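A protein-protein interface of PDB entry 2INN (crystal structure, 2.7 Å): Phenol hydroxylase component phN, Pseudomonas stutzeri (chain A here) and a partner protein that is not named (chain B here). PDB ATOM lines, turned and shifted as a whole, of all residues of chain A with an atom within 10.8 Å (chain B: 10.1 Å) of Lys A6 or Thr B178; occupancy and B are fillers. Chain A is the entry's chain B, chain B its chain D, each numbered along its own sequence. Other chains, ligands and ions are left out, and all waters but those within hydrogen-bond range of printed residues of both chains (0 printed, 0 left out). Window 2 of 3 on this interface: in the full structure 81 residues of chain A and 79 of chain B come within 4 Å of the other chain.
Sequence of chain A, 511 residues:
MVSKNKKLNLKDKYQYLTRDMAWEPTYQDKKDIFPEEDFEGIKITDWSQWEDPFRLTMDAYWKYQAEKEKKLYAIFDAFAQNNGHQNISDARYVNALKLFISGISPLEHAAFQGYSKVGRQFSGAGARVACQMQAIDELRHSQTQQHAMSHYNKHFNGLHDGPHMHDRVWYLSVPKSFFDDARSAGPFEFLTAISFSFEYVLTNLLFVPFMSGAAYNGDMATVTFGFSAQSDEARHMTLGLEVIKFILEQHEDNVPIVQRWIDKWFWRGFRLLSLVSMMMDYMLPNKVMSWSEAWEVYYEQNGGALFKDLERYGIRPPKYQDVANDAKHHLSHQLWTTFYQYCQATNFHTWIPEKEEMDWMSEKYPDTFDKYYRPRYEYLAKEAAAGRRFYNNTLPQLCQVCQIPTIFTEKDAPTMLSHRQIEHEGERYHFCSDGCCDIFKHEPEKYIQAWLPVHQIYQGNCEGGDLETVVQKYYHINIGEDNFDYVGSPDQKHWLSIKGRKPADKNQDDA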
ATOM      1  N   LYS A   6     -20.843  15.705 -29.709  1.00  0.00           N
ATOM      2  CA  LYS A   6     -20.068  16.932 -30.159  1.00  0.00           C
ATOM      3  C   LYS A   6     -18.628  16.964 -29.608  1.00  0.00           C
ATOM      4  O   LYS A   6     -17.683  17.074 -30.393  1.00  0.00           O
ATOM      5  CB  LYS A   6     -20.856  18.328 -29.933  1.00  0.00           C
ATOM      6  N   LYS A   7     -18.448  16.864 -28.287  1.00  0.00           N
ATOM      7  CA  LYS A   7     -17.084  16.844 -27.682  1.00  0.00           C
ATOM      8  C   LYS A   7     -16.907  17.914 -26.616  1.00  0.00           C
ATOM      9  O   LYS A   7     -16.835  19.072 -26.925  1.00  0.00           O
ATOM     10  CB  LYS A   7     -15.982  16.991 -28.736  1.00  0.00           C
ATOM     11  CG  LYS A   7     -14.771  16.240 -28.401  1.00  0.00           C
ATOM     12  CD  LYS A   7     -13.623  17.185 -28.457  1.00  0.00           C
ATOM     13  CE  LYS A   7     -12.395  16.533 -27.867  1.00  0.00           C
ATOM     14  NZ  LYS A   7     -11.945  15.404 -28.762  1.00  0.00           N
ATOM     15  N   LEU A   8     -16.799  17.524 -25.359  1.00  0.00           N
ATOM     16  CA  LEU A   8     -16.950  18.485 -24.261  1.00  0.00           C
ATOM     17  C   LEU A   8     -15.846  19.568 -24.087  1.00  0.00           C
ATOM     18  O   LEU A   8     -14.660  19.358 -24.358  1.00  0.00           O
ATOM     19  CB  LEU A   8     -17.178  17.712 -22.958  1.00  0.00           C
ATOM     20  CG  LEU A   8     -18.234  16.603 -23.086  1.00  0.00           C
ATOM     21  CD1 LEU A   8     -18.352  15.803 -21.782  1.00  0.00           C
ATOM     22  CD2 LEU A   8     -19.651  17.063 -23.619  1.00  0.00           C
ATOM     23  N   ASN A   9     -16.255  20.736 -23.621  1.00  0.00           N
ATOM     24  CA  ASN A   9     -15.271  21.745 -23.186  1.00  0.00           C
ATOM     25  C   ASN A   9     -14.876  21.385 -21.791  1.00  0.00           C
ATOM     26  O   ASN A   9     -15.519  20.540 -21.160  1.00  0.00           O
ATOM     27  CB  ASN A   9     -15.859  23.167 -23.213  1.00  0.00           C
ATOM     28  CG  ASN A   9     -17.305  23.191 -22.782  1.00  0.00           C
ATOM     29  OD1 ASN A   9     -17.690  22.606 -21.771  1.00  0.00           O
ATOM     30  ND2 ASN A   9     -18.105  23.845 -23.545  1.00  0.00           N
ATOM     31  N   ASP A  12     -17.705  21.404 -19.236  1.00  0.00           N
ATOM     32  CA  ASP A  12     -18.718  20.319 -19.278  1.00  0.00           C
ATOM     33  C   ASP A  12     -18.141  18.944 -18.921  1.00  0.00           C
ATOM     34  O   ASP A  12     -18.860  18.114 -18.318  1.00  0.00           O
ATOM     35  CB  ASP A  12     -19.431  20.260 -20.640  1.00  0.00           C
ATOM     36  CG  ASP A  12     -20.333  21.420 -20.859  1.00  0.00           C
ATOM     37  OD1 ASP A  12     -21.022  21.831 -19.901  1.00  0.00           O
ATOM     38  OD2 ASP A  12     -20.334  21.957 -21.984  1.00  0.00           O
ATOM     39  N   LYS A  13     -16.871  18.737 -19.306  1.00  0.00           N
ATOM     40  CA  LYS A  13     -16.164  17.530 -19.015  1.00  0.00           C
ATOM     41  C   LYS A  13     -15.859  17.423 -17.538  1.00  0.00           C
ATOM     42  O   LYS A  13     -15.696  16.319 -17.005  1.00  0.00           O
ATOM     43  CB  LYS A  13     -14.843  17.462 -19.743  1.00  0.00           C
ATOM     44  CG  LYS A  13     -14.192  16.108 -19.538  1.00  0.00           C
ATOM     45  CD  LYS A  13     -12.675  16.192 -19.664  1.00  0.00           C
ATOM     46  CE  LYS A  13     -12.025  14.810 -20.023  1.00  0.00           C
ATOM     47  NZ  LYS A  13     -11.013  15.026 -21.145  1.00  0.00           N
ATOM     48  N   TYR A  14     -15.759  18.559 -16.851  1.00  0.00           N
ATOM     49  CA  TYR A  14     -15.565  18.486 -15.424  1.00  0.00           C
ATOM     50  C   TYR A  14     -16.896  18.184 -14.730  1.00  0.00           C
ATOM     51  O   TYR A  14     -16.987  17.480 -13.679  1.00  0.00           O
ATOM     52  CB  TYR A  14     -14.994  19.767 -14.940  1.00  0.00           C
ATOM     53  CG  TYR A  14     -14.831  19.755 -13.451  1.00  0.00           C
ATOM     54  CD1 TYR A  14     -15.675  20.518 -12.586  1.00  0.00           C
ATOM     55  CD2 TYR A  14     -13.849  18.961 -12.893  1.00  0.00           C
ATOM     56  CE1 TYR A  14     -15.502  20.495 -11.300  1.00  0.00           C
ATOM     57  CE2 TYR A  14     -13.675  18.924 -11.556  1.00  0.00           C
ATOM     58  CZ  TYR A  14     -14.485  19.680 -10.766  1.00  0.00           C
ATOM     59  OH  TYR A  14     -14.226  19.519  -9.424  1.00  0.00           O
ATOM     60  N   GLN A  15     -17.945  18.712 -15.323  1.00  0.00           N
ATOM     61  CA  GLN A  15     -19.289  18.427 -14.806  1.00  0.00           C
ATOM     62  C   GLN A  15     -19.654  16.953 -14.911  1.00  0.00           C
ATOM     63  O   GLN A  15     -20.308  16.386 -13.990  1.00  0.00           O
ATOM     64  CB  GLN A  15     -20.366  19.308 -15.486  1.00  0.00           C
ATOM     65  CG  GLN A  15     -19.949  20.827 -15.550  1.00  0.00           C
ATOM     66  CD  GLN A  15     -21.003  21.846 -15.019  1.00  0.00           C
ATOM     67  OE1 GLN A  15     -20.678  22.817 -14.282  1.00  0.00           O
ATOM     68  NE2 GLN A  15     -22.249  21.626 -15.411  1.00  0.00           N
ATOM     69  N   TYR A  16     -19.267  16.352 -16.031  1.00  0.00           N
ATOM     70  CA  TYR A  16     -19.578  14.970 -16.219  1.00  0.00           C
ATOM     71  C   TYR A  16     -18.761  14.184 -15.236  1.00  0.00           C
ATOM     72  O   TYR A  16     -19.159  13.110 -14.779  1.00  0.00           O
ATOM     73  CB  TYR A  16     -19.314  14.501 -17.644  1.00  0.00           C
ATOM     74  CG  TYR A  16     -20.597  14.351 -18.483  1.00  0.00           C
ATOM     75  CD1 TYR A  16     -20.780  15.091 -19.656  1.00  0.00           C
ATOM     76  CD2 TYR A  16     -21.630  13.476 -18.105  1.00  0.00           C
ATOM     77  CE1 TYR A  16     -21.941  15.016 -20.442  1.00  0.00           C
ATOM     78  CE2 TYR A  16     -22.822  13.347 -18.949  1.00  0.00           C
ATOM     79  CZ  TYR A  16     -22.949  14.162 -20.115  1.00  0.00           C
ATOM     80  OH  TYR A  16     -24.039  14.086 -20.945  1.00  0.00           O
ATOM     81  N   LEU A  17     -17.634  14.744 -14.870  1.00  0.00           N
ATOM     82  CA  LEU A  17     -16.787  14.071 -13.968  1.00  0.00           C
ATOM     83  C   LEU A  17     -17.208  14.350 -12.529  1.00  0.00           C
ATOM     84  O   LEU A  17     -16.558  13.968 -11.577  1.00  0.00           O
ATOM     85  CB  LEU A  17     -15.330  14.430 -14.299  1.00  0.00           C
ATOM     86  CG  LEU A  17     -14.463  13.284 -14.922  1.00  0.00           C
ATOM     87  CD1 LEU A  17     -15.189  11.976 -15.248  1.00  0.00           C
ATOM     88  CD2 LEU A  17     -13.679  13.665 -16.158  1.00  0.00           C
ATOM     89  N   ASP A  20     -22.561  14.896 -12.722  1.00  0.00           N
ATOM     90  CA  ASP A  20     -23.405  13.873 -13.395  1.00  0.00           C
ATOM     91  C   ASP A  20     -23.457  12.503 -12.700  1.00  0.00           C
ATOM     92  O   ASP A  20     -24.278  11.660 -13.042  1.00  0.00           O
ATOM     93  CB  ASP A  20     -23.049  13.758 -14.893  1.00  0.00           C
ATOM     94  CG  ASP A  20     -23.804  12.631 -15.630  1.00  0.00           C
ATOM     95  OD1 ASP A  20     -23.120  11.626 -15.919  1.00  0.00           O
ATOM     96  OD2 ASP A  20     -25.020  12.756 -15.973  1.00  0.00           O
ATOM     97  N   THR B 109     -12.211   1.552 -27.886  1.00  0.00           N
ATOM     98  CA  THR B 109     -13.046   2.032 -28.965  1.00  0.00           C
ATOM     99  C   THR B 109     -13.024   1.016 -30.084  1.00  0.00           C
ATOM    100  O   THR B 109     -13.833   1.109 -31.042  1.00  0.00           O
ATOM    101  CB  THR B 109     -12.567   3.421 -29.547  1.00  0.00           C
ATOM    102  OG1 THR B 109     -11.142   3.379 -29.833  1.00  0.00           O
ATOM    103  CG2 THR B 109     -12.951   4.611 -28.597  1.00  0.00           C
ATOM    104  N   SER B 168     -16.110   6.769 -14.449  1.00  0.00           N
ATOM    105  CA  SER B 168     -16.684   7.726 -15.360  1.00  0.00           C
ATOM    106  C   SER B 168     -15.767   7.785 -16.588  1.00  0.00           C
ATOM    107  O   SER B 168     -16.258   7.846 -17.739  1.00  0.00           O
ATOM    108  CB  SER B 168     -16.842   9.107 -14.718  1.00  0.00           C
ATOM    109  OG  SER B 168     -17.167   9.109 -13.309  1.00  0.00           O
ATOM    110  N   ARG B 169     -14.451   7.729 -16.392  1.00  0.00           N
ATOM    111  CA  ARG B 169     -13.576   7.895 -17.549  1.00  0.00           C
ATOM    112  C   ARG B 169     -13.468   6.720 -18.504  1.00  0.00           C
ATOM    113  O   ARG B 169     -13.129   6.911 -19.687  1.00  0.00           O
ATOM    114  CB  ARG B 169     -12.172   8.348 -17.161  1.00  0.00           C
ATOM    115  CG  ARG B 169     -12.021   9.791 -16.787  1.00  0.00           C
ATOM    116  CD  ARG B 169     -10.663  10.054 -17.204  1.00  0.00           C
ATOM    117  NE  ARG B 169      -9.839  10.156 -16.024  1.00  0.00           N
ATOM    118  CZ  ARG B 169      -8.510  10.055 -15.998  1.00  0.00           C
ATOM    119  NH1 ARG B 169      -7.795   9.768 -17.081  1.00  0.00           N
ATOM    120  NH2 ARG B 169      -7.889  10.212 -14.830  1.00  0.00           N
ATOM    121  N   ILE B 170     -13.717   5.508 -18.031  1.00  0.00           N
ATOM    122  CA  ILE B 170     -13.792   4.424 -18.986  1.00  0.00           C
ATOM    123  C   ILE B 170     -14.829   4.778 -20.101  1.00  0.00           C
ATOM    124  O   ILE B 170     -14.525   4.627 -21.312  1.00  0.00           O
ATOM    125  CB  ILE B 170     -14.119   3.076 -18.352  1.00  0.00           C
ATOM    126  CG1 ILE B 170     -13.048   2.628 -17.328  1.00  0.00           C
ATOM    127  CG2 ILE B 170     -14.247   2.012 -19.450  1.00  0.00           C
ATOM    128  CD1 ILE B 170     -13.679   1.936 -16.087  1.00  0.00           C
ATOM    129  N   ALA B 171     -16.013   5.256 -19.701  1.00  0.00           N
ATOM    130  CA  ALA B 171     -17.016   5.773 -20.601  1.00  0.00           C
ATOM    131  C   ALA B 171     -16.485   6.910 -21.415  1.00  0.00           C
ATOM    132  O   ALA B 171     -16.620   6.897 -22.617  1.00  0.00           O
ATOM    133  CB  ALA B 171     -18.244   6.225 -19.865  1.00  0.00           C
ATOM    134  N   LEU B 172     -15.864   7.920 -20.864  1.00  0.00           N
ATOM    135  CA  LEU B 172     -15.470   8.916 -21.880  1.00  0.00           C
ATOM    136  C   LEU B 172     -14.562   8.347 -22.947  1.00  0.00           C
ATOM    137  O   LEU B 172     -14.640   8.762 -24.093  1.00  0.00           O
ATOM    138  CB  LEU B 172     -14.951  10.263 -21.328  1.00  0.00           C
ATOM    139  CG  LEU B 172     -15.905  10.780 -20.276  1.00  0.00           C
ATOM    140  CD1 LEU B 172     -15.297  11.982 -19.609  1.00  0.00           C
ATOM    141  CD2 LEU B 172     -17.301  11.069 -20.850  1.00  0.00           C
ATOM    142  N   MET B 173     -13.699   7.411 -22.577  1.00  0.00           N
ATOM    143  CA  MET B 173     -12.844   6.775 -23.575  1.00  0.00           C
ATOM    144  C   MET B 173     -13.672   6.054 -24.653  1.00  0.00           C
ATOM    145  O   MET B 173     -13.414   6.163 -25.848  1.00  0.00           O
ATOM    146  CB  MET B 173     -11.877   5.833 -22.908  1.00  0.00           C
ATOM    147  CG  MET B 173     -10.976   5.145 -23.841  1.00  0.00           C
ATOM    148  SD  MET B 173      -9.414   4.277 -22.929  1.00  0.00           S
ATOM    149  CE  MET B 173      -9.196   5.430 -21.345  1.00  0.00           C
ATOM    150  N   ILE B 174     -14.717   5.353 -24.233  1.00  0.00           N
ATOM    151  CA  ILE B 174     -15.642   4.742 -25.166  1.00  0.00           C
ATOM    152  C   ILE B 174     -16.440   5.689 -26.066  1.00  0.00           C
ATOM    153  O   ILE B 174     -16.715   5.375 -27.190  1.00  0.00           O
ATOM    154  CB  ILE B 174     -16.641   3.879 -24.411  1.00  0.00           C
ATOM    155  CG1 ILE B 174     -15.912   2.808 -23.604  1.00  0.00           C
ATOM    156  CG2 ILE B 174     -17.640   3.263 -25.387  1.00  0.00           C
ATOM    157  CD1 ILE B 174     -16.806   2.099 -22.675  1.00  0.00           C
ATOM    158  N   ASP B 175     -16.881   6.820 -25.583  1.00  0.00           N
ATOM    159  CA  ASP B 175     -17.629   7.648 -26.449  1.00  0.00           C
ATOM    160  C   ASP B 175     -16.795   8.779 -26.997  1.00  0.00           C
ATOM    161  O   ASP B 175     -17.296   9.598 -27.771  1.00  0.00           O
ATOM    162  CB  ASP B 175     -18.853   8.164 -25.722  1.00  0.00           C
ATOM    163  CG  ASP B 175     -18.547   9.259 -24.699  1.00  0.00           C
ATOM    164  OD1 ASP B 175     -17.662  10.128 -24.937  1.00  0.00           O
ATOM    165  OD2 ASP B 175     -19.270   9.265 -23.669  1.00  0.00           O
ATOM    166  N   GLY B 176     -15.523   8.824 -26.575  1.00  0.00           N
ATOM    167  CA  GLY B 176     -14.480   9.676 -27.157  1.00  0.00           C
ATOM    168  C   GLY B 176     -14.767  11.080 -26.705  1.00  0.00           C
ATOM    169  O   GLY B 176     -14.645  12.014 -27.479  1.00  0.00           O
ATOM    170  N   SER B 177     -15.165  11.236 -25.449  1.00  0.00           N
ATOM    171  CA  SER B 177     -15.312  12.562 -24.861  1.00  0.00           C
ATOM    172  C   SER B 177     -16.571  13.367 -25.278  1.00  0.00           C
ATOM    173  O   SER B 177     -16.682  14.551 -24.967  1.00  0.00           O
ATOM    174  CB  SER B 177     -14.030  13.380 -25.031  1.00  0.00           C
ATOM    175  OG  SER B 177     -13.624  13.948 -23.797  1.00  0.00           O
ATOM    176  N   THR B 178     -17.523  12.689 -25.922  1.00  0.00           N
ATOM    177  CA  THR B 178     -18.895  13.171 -26.124  1.00  0.00           C
ATOM    178  C   THR B 178     -19.773  13.117 -24.876  1.00  0.00           C
ATOM    179  O   THR B 178     -20.632  14.012 -24.654  1.00  0.00           O
ATOM    180  CB  THR B 178     -19.549  12.243 -27.093  1.00  0.00           C
ATOM    181  OG1 THR B 178     -18.617  12.022 -28.137  1.00  0.00           O
ATOM    182  CG2 THR B 178     -20.863  12.826 -27.729  1.00  0.00           C
ATOM    183  N   GLY B 179     -19.611  12.079 -24.064  1.00  0.00           N
ATOM    184  CA  GLY B 179     -20.437  11.983 -22.863  1.00  0.00           C
ATOM    185  C   GLY B 179     -21.765  11.322 -23.099  1.00  0.00           C
ATOM    186  O   GLY B 179     -22.610  11.315 -22.232  1.00  0.00           O
ATOM    187  N   ALA B 180     -21.962  10.768 -24.281  1.00  0.00           N
ATOM    188  CA  ALA B 180     -23.140   9.960 -24.584  1.00  0.00           C
ATOM    189  C   ALA B 180     -23.146   8.575 -23.879  1.00  0.00           C
ATOM    190  O   ALA B 180     -24.225   8.029 -23.619  1.00  0.00           O
ATOM    191  CB  ALA B 180     -23.251   9.779 -26.126  1.00  0.00           C
ATOM    192  N   ALA B 181     -21.952   8.025 -23.601  1.00  0.00           N
ATOM    193  CA  ALA B 181     -21.804   6.720 -22.904  1.00  0.00           C
ATOM    194  C   ALA B 181     -22.128   6.930 -21.450  1.00  0.00           C
ATOM    195  O   ALA B 181     -22.747   6.088 -20.768  1.00  0.00           O
ATOM    196  CB  ALA B 181     -20.406   6.178 -23.012  1.00  0.00           C
ATOM    197  N   LEU B 182     -21.676   8.074 -20.958  1.00  0.00           N
ATOM    198  CA  LEU B 182     -22.046   8.499 -19.634  1.00  0.00           C
ATOM    199  C   LEU B 182     -23.569   8.530 -19.543  1.00  0.00           C
ATOM    200  O   LEU B 182     -24.174   8.003 -18.566  1.00  0.00           O
ATOM    201  CB  LEU B 182     -21.384   9.828 -19.341  1.00  0.00           C
ATOM    202  CG  LEU B 182     -20.328   9.779 -18.231  1.00  0.00           C
ATOM    203  CD1 LEU B 182     -19.809   8.400 -17.901  1.00  0.00           C
ATOM    204  CD2 LEU B 182     -19.191  10.731 -18.531  1.00  0.00           C
ATOM    205  N   ASP B 183     -24.198   9.078 -20.580  1.00  0.00           N
ATOM    206  CA  ASP B 183     -25.631   9.087 -20.614  1.00  0.00           C
ATOM    207  C   ASP B 183     -26.321   7.705 -20.778  1.00  0.00           C
ATOM    208  O   ASP B 183     -27.252   7.364 -19.975  1.00  0.00           O
ATOM    209  CB  ASP B 183     -26.097  10.073 -21.637  1.00  0.00           C
ATOM    210  CG  ASP B 183     -25.935  11.450 -21.154  1.00  0.00           C
ATOM    211  OD1 ASP B 183     -25.912  11.679 -19.897  1.00  0.00           O
ATOM    212  OD2 ASP B 183     -25.805  12.309 -22.021  1.00  0.00           O
ATOM    213  N   GLU B 184     -25.899   6.914 -21.774  1.00  0.00           N
ATOM    214  CA  GLU B 184     -26.465   5.601 -21.874  1.00  0.00           C
ATOM    215  C   GLU B 184     -26.357   4.868 -20.531  1.00  0.00           C
ATOM    216  O   GLU B 184     -27.363   4.312 -20.037  1.00  0.00           O
ATOM    217  CB  GLU B 184     -25.789   4.821 -22.950  1.00  0.00           C
ATOM    218  CG  GLU B 184     -26.316   3.438 -23.096  1.00  0.00           C
ATOM    219  CD  GLU B 184     -25.489   2.659 -24.093  1.00  0.00           C
ATOM    220  OE1 GLU B 184     -24.747   3.305 -24.823  1.00  0.00           O
ATOM    221  OE2 GLU B 184     -25.553   1.411 -24.125  1.00  0.00           O
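The backbone NH (N) of Leu A8 is in hydrogen-bond range of the backbone carbonyl oxygen (O) of Ser B177.
OD2 of Asp B183 lies within hydrogen-bond range of OH of Tyr A16, at 2.7 Å.
O of Gly B179 is in hydrogen-bond range of OH of Tyr A16 (3.4 Å).
The side-chain carboxylate (OD2) of Asp B175 is in hydrogen-bond range of the backbone NH (N) of Gly B179 (2.9 Å).
The backbone NH (N) of Ser B177 lies within hydrogen-bond range of the backbone carbonyl oxygen (O) of Leu B172 (2.9 Å).
The side-chain carboxylate (OD1) of Asp B175 is in hydrogen-bond range of the backbone NH (N) of Ser B177 (2.8 Å).
The side-chain carboxylate of Asp B175 lies within hydrogen-bond range of the backbone NH of Thr B178 (2.7 Å).
Among the printed residues, merely in contact across the chains: Leu A17 with Ser B168, Leu A8 with Thr B178, Lys A6 with Thr B178, Lys A7 with Ser B177, Tyr A16 with Leu B182 and Lys A13 with Ser B177.
Of chain B, only Thr B178 comes within 4 Å of Lys A6.
Of the printed residues of chain B, Lys A13 touches Ser B177 (3.9 Å).
Gln A15 touches none of the printed residues of chain B.
No residue of chain A comes within 4 Å of Asp B175.
Thr B178 touches just these residues of chain A: Lys A6 (3.5 Å) and Leu A8 (3.4 Å).
Gly B179 touches just one residue of chain A: Tyr A16.
Printed residues of chain A within 4 Å of Asp B183: Tyr A16.
The nearest residue of chain B that does not touch Lys A6 is Ser B177 (5.6 Å).
The nearest residue of chain A that does not touch Thr B178 is Lys A7 (4.3 Å).
The nearest printed residue of chain B that does not touch Tyr A16 is Thr B178 (4.5 Å).
Hydrophobic or aromatic side chains of chain A that line the printed part of chain B: Leu A8, Tyr A16 and Leu A17.
Hydrophobic or aromatic side chains of chain B within 4 Å of the printed part of chain A: Leu B182.
Among the printed residues, 9 pairs touch across the chains.
Among the printed residues, no Asp or Glu carboxylate lies within 4 Å of a Lys or Arg side-chain nitrogen of the other chain.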
